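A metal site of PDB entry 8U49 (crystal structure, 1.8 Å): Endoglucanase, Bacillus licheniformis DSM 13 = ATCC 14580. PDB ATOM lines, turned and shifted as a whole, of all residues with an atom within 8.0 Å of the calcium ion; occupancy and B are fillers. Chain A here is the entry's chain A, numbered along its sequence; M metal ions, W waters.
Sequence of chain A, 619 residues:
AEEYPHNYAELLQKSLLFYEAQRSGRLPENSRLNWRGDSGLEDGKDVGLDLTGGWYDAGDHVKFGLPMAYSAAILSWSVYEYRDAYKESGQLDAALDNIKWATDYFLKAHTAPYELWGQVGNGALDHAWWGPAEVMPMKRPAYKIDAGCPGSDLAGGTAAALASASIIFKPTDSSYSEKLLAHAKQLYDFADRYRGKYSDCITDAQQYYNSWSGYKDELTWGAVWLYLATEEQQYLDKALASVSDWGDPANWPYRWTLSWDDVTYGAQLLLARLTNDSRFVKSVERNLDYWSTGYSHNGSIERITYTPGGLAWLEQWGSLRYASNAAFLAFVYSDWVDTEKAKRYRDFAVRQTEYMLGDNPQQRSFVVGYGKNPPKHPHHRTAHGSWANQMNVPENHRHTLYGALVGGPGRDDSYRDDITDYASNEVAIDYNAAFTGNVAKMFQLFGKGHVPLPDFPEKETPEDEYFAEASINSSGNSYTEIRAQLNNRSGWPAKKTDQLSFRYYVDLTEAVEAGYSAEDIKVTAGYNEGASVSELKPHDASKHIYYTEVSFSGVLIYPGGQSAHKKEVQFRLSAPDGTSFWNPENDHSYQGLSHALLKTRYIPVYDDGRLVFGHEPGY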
ATOM      1  N   THR A 480      -1.867  -5.971  26.566  1.00  0.00           N
ATOM      2  CA  THR A 480      -2.888  -6.243  27.571  1.00  0.00           C
ATOM      3  C   THR A 480      -3.050  -4.987  28.409  1.00  0.00           C
ATOM      4  O   THR A 480      -2.046  -4.402  28.848  1.00  0.00           O
ATOM      5  CB  THR A 480      -2.517  -7.404  28.494  1.00  0.00           C
ATOM      6  OG1 THR A 480      -2.380  -8.613  27.749  1.00  0.00           O
ATOM      7  CG2 THR A 480      -3.584  -7.601  29.583  1.00  0.00           C
ATOM      8  N   TYR A 505       2.563 -10.167  36.716  1.00  0.00           N
ATOM      9  CA  TYR A 505       3.573 -11.035  36.144  1.00  0.00           C
ATOM     10  C   TYR A 505       3.181 -11.509  34.757  1.00  0.00           C
ATOM     11  O   TYR A 505       2.037 -11.916  34.538  1.00  0.00           O
ATOM     12  CB  TYR A 505       3.793 -12.250  37.035  1.00  0.00           C
ATOM     13  CG  TYR A 505       4.488 -11.958  38.326  1.00  0.00           C
ATOM     14  CD1 TYR A 505       3.770 -11.542  39.447  1.00  0.00           C
ATOM     15  CD2 TYR A 505       5.863 -12.065  38.436  1.00  0.00           C
ATOM     16  CE1 TYR A 505       4.428 -11.267  40.648  1.00  0.00           C
ATOM     17  CE2 TYR A 505       6.513 -11.801  39.622  1.00  0.00           C
ATOM     18  CZ  TYR A 505       5.800 -11.413  40.719  1.00  0.00           C
ATOM     19  OH  TYR A 505       6.456 -11.134  41.890  1.00  0.00           O
ATOM     20  N   VAL A 506       4.158 -11.500  33.838  1.00  0.00           N
ATOM     21  CA  VAL A 506       3.955 -11.964  32.465  1.00  0.00           C
ATOM     22  C   VAL A 506       5.030 -12.987  32.137  1.00  0.00           C
ATOM     23  O   VAL A 506       6.097 -13.039  32.752  1.00  0.00           O
ATOM     24  CB  VAL A 506       3.970 -10.813  31.433  1.00  0.00           C
ATOM     25  CG1 VAL A 506       2.851  -9.810  31.704  1.00  0.00           C
ATOM     26  CG2 VAL A 506       5.333 -10.104  31.426  1.00  0.00           C
ATOM     27  N   ASP A 507       4.720 -13.830  31.159  1.00  0.00           N
ATOM     28  CA  ASP A 507       5.689 -14.734  30.542  1.00  0.00           C
ATOM     29  C   ASP A 507       6.012 -14.171  29.170  1.00  0.00           C
ATOM     30  O   ASP A 507       5.109 -13.981  28.348  1.00  0.00           O
ATOM     31  CB  ASP A 507       5.104 -16.145  30.433  1.00  0.00           C
ATOM     32  CG  ASP A 507       6.104 -17.177  29.908  1.00  0.00           C
ATOM     33  OD1 ASP A 507       7.119 -16.814  29.273  1.00  0.00           O
ATOM     34  OD2 ASP A 507       5.847 -18.379  30.135  1.00  0.00           O
ATOM     35  N   LEU A 508       7.297 -13.870  28.931  1.00  0.00           N
ATOM     36  CA  LEU A 508       7.713 -13.313  27.658  1.00  0.00           C
ATOM     37  C   LEU A 508       8.318 -14.360  26.719  1.00  0.00           C
ATOM     38  O   LEU A 508       9.027 -13.980  25.774  1.00  0.00           O
ATOM     39  CB  LEU A 508       8.697 -12.174  27.861  1.00  0.00           C
ATOM     40  CG  LEU A 508       8.126 -10.984  28.627  1.00  0.00           C
ATOM     41  CD1 LEU A 508       9.116  -9.827  28.602  1.00  0.00           C
ATOM     42  CD2 LEU A 508       6.790 -10.578  28.015  1.00  0.00           C
ATOM     43  N   THR A 509       8.054 -15.648  26.946  1.00  0.00           N
ATOM     44  CA  THR A 509       8.630 -16.666  26.074  1.00  0.00           C
ATOM     45  C   THR A 509       8.264 -16.420  24.618  1.00  0.00           C
ATOM     46  O   THR A 509       9.112 -16.557  23.723  1.00  0.00           O
ATOM     47  CB  THR A 509       8.179 -18.064  26.517  1.00  0.00           C
ATOM     48  OG1 THR A 509       8.704 -18.353  27.806  1.00  0.00           O
ATOM     49  CG2 THR A 509       8.697 -19.114  25.537  1.00  0.00           C
ATOM     50  N   GLU A 510       7.008 -16.052  24.348  1.00  0.00           N
ATOM     51  CA  GLU A 510       6.617 -15.822  22.962  1.00  0.00           C
ATOM     52  C   GLU A 510       7.312 -14.600  22.372  1.00  0.00           C
ATOM     53  O   GLU A 510       7.580 -14.563  21.165  1.00  0.00           O
ATOM     54  CB  GLU A 510       5.096 -15.700  22.849  1.00  0.00           C
ATOM     55  CG  GLU A 510       4.516 -14.364  23.329  1.00  0.00           C
ATOM     56  CD  GLU A 510       4.141 -14.354  24.807  1.00  0.00           C
ATOM     57  OE1 GLU A 510       4.384 -15.357  25.522  1.00  0.00           O
ATOM     58  OE2 GLU A 510       3.599 -13.325  25.256  1.00  0.00           O
ATOM     59  N   ALA A 511       7.641 -13.606  23.211  1.00  0.00           N
ATOM     60  CA  ALA A 511       8.422 -12.463  22.738  1.00  0.00           C
ATOM     61  C   ALA A 511       9.827 -12.885  22.337  1.00  0.00           C
ATOM     62  O   ALA A 511      10.313 -12.527  21.241  1.00  0.00           O
ATOM     63  CB  ALA A 511       8.471 -11.376  23.823  1.00  0.00           C
ATOM     64  N   HIS A 544      11.909 -16.571  31.327  1.00  0.00           N
ATOM     65  CA  HIS A 544      11.423 -15.325  30.734  1.00  0.00           C
ATOM     66  C   HIS A 544      10.201 -14.789  31.467  1.00  0.00           C
ATOM     67  O   HIS A 544       9.265 -14.297  30.831  1.00  0.00           O
ATOM     68  CB  HIS A 544      11.128 -15.503  29.245  1.00  0.00           C
ATOM     69  CG  HIS A 544      12.241 -16.141  28.491  1.00  0.00           C
ATOM     70  ND1 HIS A 544      13.473 -15.543  28.327  1.00  0.00           N
ATOM     71  CD2 HIS A 544      12.312 -17.332  27.858  1.00  0.00           C
ATOM     72  CE1 HIS A 544      14.252 -16.337  27.622  1.00  0.00           C
ATOM     73  NE2 HIS A 544      13.576 -17.431  27.317  1.00  0.00           N
ATOM     74  N   ILE A 545      10.209 -14.857  32.789  1.00  0.00           N
ATOM     75  CA  ILE A 545       9.111 -14.339  33.597  1.00  0.00           C
ATOM     76  C   ILE A 545       9.501 -12.963  34.108  1.00  0.00           C
ATOM     77  O   ILE A 545      10.554 -12.807  34.728  1.00  0.00           O
ATOM     78  CB  ILE A 545       8.762 -15.274  34.763  1.00  0.00           C
ATOM     79  CG1 ILE A 545       8.559 -16.722  34.271  1.00  0.00           C
ATOM     80  CG2 ILE A 545       7.498 -14.792  35.477  1.00  0.00           C
ATOM     81  CD1 ILE A 545       7.544 -16.872  33.146  1.00  0.00           C
ATOM     82  N   PHE A 581       3.124 -10.999  18.328  1.00  0.00           N
ATOM     83  CA  PHE A 581       3.507 -12.129  19.150  1.00  0.00           C
ATOM     84  C   PHE A 581       2.848 -12.146  20.519  1.00  0.00           C
ATOM     85  O   PHE A 581       2.739 -13.223  21.120  1.00  0.00           O
ATOM     86  CB  PHE A 581       5.030 -12.171  19.329  1.00  0.00           C
ATOM     87  CG  PHE A 581       5.594 -10.935  19.975  1.00  0.00           C
ATOM     88  CD1 PHE A 581       5.484 -10.745  21.346  1.00  0.00           C
ATOM     89  CD2 PHE A 581       6.257  -9.986  19.219  1.00  0.00           C
ATOM     90  CE1 PHE A 581       5.997  -9.616  21.952  1.00  0.00           C
ATOM     91  CE2 PHE A 581       6.782  -8.845  19.822  1.00  0.00           C
ATOM     92  CZ  PHE A 581       6.655  -8.672  21.188  1.00  0.00           C
ATOM     93  N   TRP A 582       2.408 -10.996  21.037  1.00  0.00           N
ATOM     94  CA  TRP A 582       1.988 -10.891  22.430  1.00  0.00           C
ATOM     95  C   TRP A 582       0.887 -11.888  22.769  1.00  0.00           C
ATOM     96  O   TRP A 582      -0.133 -11.970  22.072  1.00  0.00           O
ATOM     97  CB  TRP A 582       1.504  -9.462  22.723  1.00  0.00           C
ATOM     98  CG  TRP A 582       1.059  -9.208  24.146  1.00  0.00           C
ATOM     99  CD1 TRP A 582      -0.226  -9.190  24.606  1.00  0.00           C
ATOM    100  CD2 TRP A 582       1.903  -8.936  25.287  1.00  0.00           C
ATOM    101  NE1 TRP A 582      -0.237  -8.912  25.961  1.00  0.00           N
ATOM    102  CE2 TRP A 582       1.053  -8.764  26.396  1.00  0.00           C
ATOM    103  CE3 TRP A 582       3.282  -8.831  25.460  1.00  0.00           C
ATOM    104  CZ2 TRP A 582       1.540  -8.478  27.682  1.00  0.00           C
ATOM    105  CZ3 TRP A 582       3.779  -8.547  26.742  1.00  0.00           C
ATOM    106  CH2 TRP A 582       2.899  -8.366  27.834  1.00  0.00           C
ATOM    107  N   ASN A 583       1.103 -12.674  23.829  1.00  0.00           N
ATOM    108  CA  ASN A 583       0.188 -13.739  24.229  1.00  0.00           C
ATOM    109  C   ASN A 583      -0.040 -13.688  25.738  1.00  0.00           C
ATOM    110  O   ASN A 583       0.796 -14.163  26.509  1.00  0.00           O
ATOM    111  CB  ASN A 583       0.704 -15.111  23.816  1.00  0.00           C
ATOM    112  CG  ASN A 583      -0.222 -16.234  24.239  1.00  0.00           C
ATOM    113  OD1 ASN A 583      -1.363 -15.997  24.654  1.00  0.00           O
ATOM    114  ND2 ASN A 583       0.248 -17.474  24.121  1.00  0.00           N
ATOM    115  N   PRO A 584      -1.176 -13.163  26.185  1.00  0.00           N
ATOM    116  CA  PRO A 584      -1.403 -13.069  27.633  1.00  0.00           C
ATOM    117  C   PRO A 584      -1.733 -14.412  28.280  1.00  0.00           C
ATOM    118  O   PRO A 584      -1.677 -14.524  29.508  1.00  0.00           O
ATOM    119  CB  PRO A 584      -2.600 -12.115  27.739  1.00  0.00           C
ATOM    120  CG  PRO A 584      -3.379 -12.397  26.479  1.00  0.00           C
ATOM    121  CD  PRO A 584      -2.331 -12.688  25.406  1.00  0.00           C
ATOM    122  N   GLU A 585      -2.079 -15.428  27.484  1.00  0.00           N
ATOM    123  CA  GLU A 585      -2.641 -16.639  28.065  1.00  0.00           C
ATOM    124  C   GLU A 585      -1.636 -17.419  28.889  1.00  0.00           C
ATOM    125  O   GLU A 585      -2.049 -18.240  29.714  1.00  0.00           O
ATOM    126  CB  GLU A 585      -3.224 -17.539  26.966  1.00  0.00           C
ATOM    127  CG  GLU A 585      -4.287 -16.875  26.070  1.00  0.00           C
ATOM    128  CD  GLU A 585      -5.536 -16.424  26.826  1.00  0.00           C
ATOM    129  OE1 GLU A 585      -5.935 -17.070  27.819  1.00  0.00           O
ATOM    130  OE2 GLU A 585      -6.121 -15.393  26.418  1.00  0.00           O
ATOM    131  N   ASN A 586      -0.327 -17.210  28.690  1.00  0.00           N
ATOM    132  CA  ASN A 586       0.667 -17.836  29.546  1.00  0.00           C
ATOM    133  C   ASN A 586       1.163 -16.914  30.641  1.00  0.00           C
ATOM    134  O   ASN A 586       2.159 -17.241  31.311  1.00  0.00           O
ATOM    135  CB  ASN A 586       1.842 -18.371  28.716  1.00  0.00           C
ATOM    136  CG  ASN A 586       2.525 -17.313  27.865  1.00  0.00           C
ATOM    137  OD1 ASN A 586       2.343 -16.117  28.059  1.00  0.00           O
ATOM    138  ND2 ASN A 586       3.318 -17.757  26.886  1.00  0.00           N
ATOM    139  N   ASP A 587       0.497 -15.776  30.861  1.00  0.00           N
ATOM    140  CA  ASP A 587       0.932 -14.797  31.855  1.00  0.00           C
ATOM    141  C   ASP A 587       0.323 -15.126  33.217  1.00  0.00           C
ATOM    142  O   ASP A 587      -0.899 -15.267  33.338  1.00  0.00           O
ATOM    143  CB  ASP A 587       0.554 -13.370  31.437  1.00  0.00           C
ATOM    144  CG  ASP A 587       1.325 -12.884  30.204  1.00  0.00           C
ATOM    145  OD1 ASP A 587       2.246 -13.588  29.733  1.00  0.00           O
ATOM    146  OD2 ASP A 587       1.008 -11.787  29.717  1.00  0.00           O
ATOM    147  N   HIS A 588       1.190 -15.218  34.227  1.00  0.00           N
ATOM    148  CA  HIS A 588       0.774 -15.616  35.575  1.00  0.00           C
ATOM    149  C   HIS A 588      -0.374 -14.751  36.096  1.00  0.00           C
ATOM    150  O   HIS A 588      -1.387 -15.264  36.562  1.00  0.00           O
ATOM    151  CB  HIS A 588       1.991 -15.551  36.498  1.00  0.00           C
ATOM    152  CG  HIS A 588       1.673 -15.758  37.949  1.00  0.00           C
ATOM    153  ND1 HIS A 588       1.687 -17.004  38.544  1.00  0.00           N
ATOM    154  CD2 HIS A 588       1.360 -14.876  38.926  1.00  0.00           C
ATOM    155  CE1 HIS A 588       1.389 -16.881  39.832  1.00  0.00           C
ATOM    156  NE2 HIS A 588       1.185 -15.598  40.087  1.00  0.00           N
ATOM    157  N   TYR A 590      -2.483 -12.843  34.500  1.00  0.00           N
ATOM    158  CA  TYR A 590      -3.647 -12.801  33.619  1.00  0.00           C
ATOM    159  C   TYR A 590      -4.661 -13.908  33.902  1.00  0.00           C
ATOM    160  O   TYR A 590      -5.801 -13.819  33.447  1.00  0.00           O
ATOM    161  CB  TYR A 590      -3.173 -12.898  32.171  1.00  0.00           C
ATOM    162  CG  TYR A 590      -4.155 -12.519  31.089  1.00  0.00           C
ATOM    163  CD1 TYR A 590      -4.443 -11.184  30.824  1.00  0.00           C
ATOM    164  CD2 TYR A 590      -4.737 -13.482  30.275  1.00  0.00           C
ATOM    165  CE1 TYR A 590      -5.316 -10.818  29.808  1.00  0.00           C
ATOM    166  CE2 TYR A 590      -5.609 -13.137  29.246  1.00  0.00           C
ATOM    167  CZ  TYR A 590      -5.886 -11.795  29.025  1.00  0.00           C
ATOM    168  OH  TYR A 590      -6.737 -11.427  28.008  1.00  0.00           O
HETATM  169 CA    CA M   1       3.002 -14.014  27.416  1.00  0.00          CA
HETATM  170  O   HOH W   1       2.671 -11.620  27.545  1.00  0.00           O
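The side-chain carboxylate (OD1) of Asp 507 is in hydrogen-bond range of the side-chain hydroxyl (OG1) of Thr 509, 2.7 Å away.
The side-chain amide oxygen of Asn 583 is in hydrogen-bond range of the backbone NH of Glu 585.
Five residues have an atom within 4 Å of the calcium ion: Asp 507, Glu 510, Asn 583, Asn 586 and Asp 587.
The calcium ion is bound by OD1 of Asn 586 (2.3 Å), O of Asp 507 (2.3 Å), OE2 of Glu 510 (2.3 Å), O of Asn 583 (2.4 Å), water W1 (2.4 Å), OD1 of Asp 587 (2.5 Å) and OE1 of Glu 510 (2.7 Å).
The calcium ion has seven donor atoms within binding distance.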
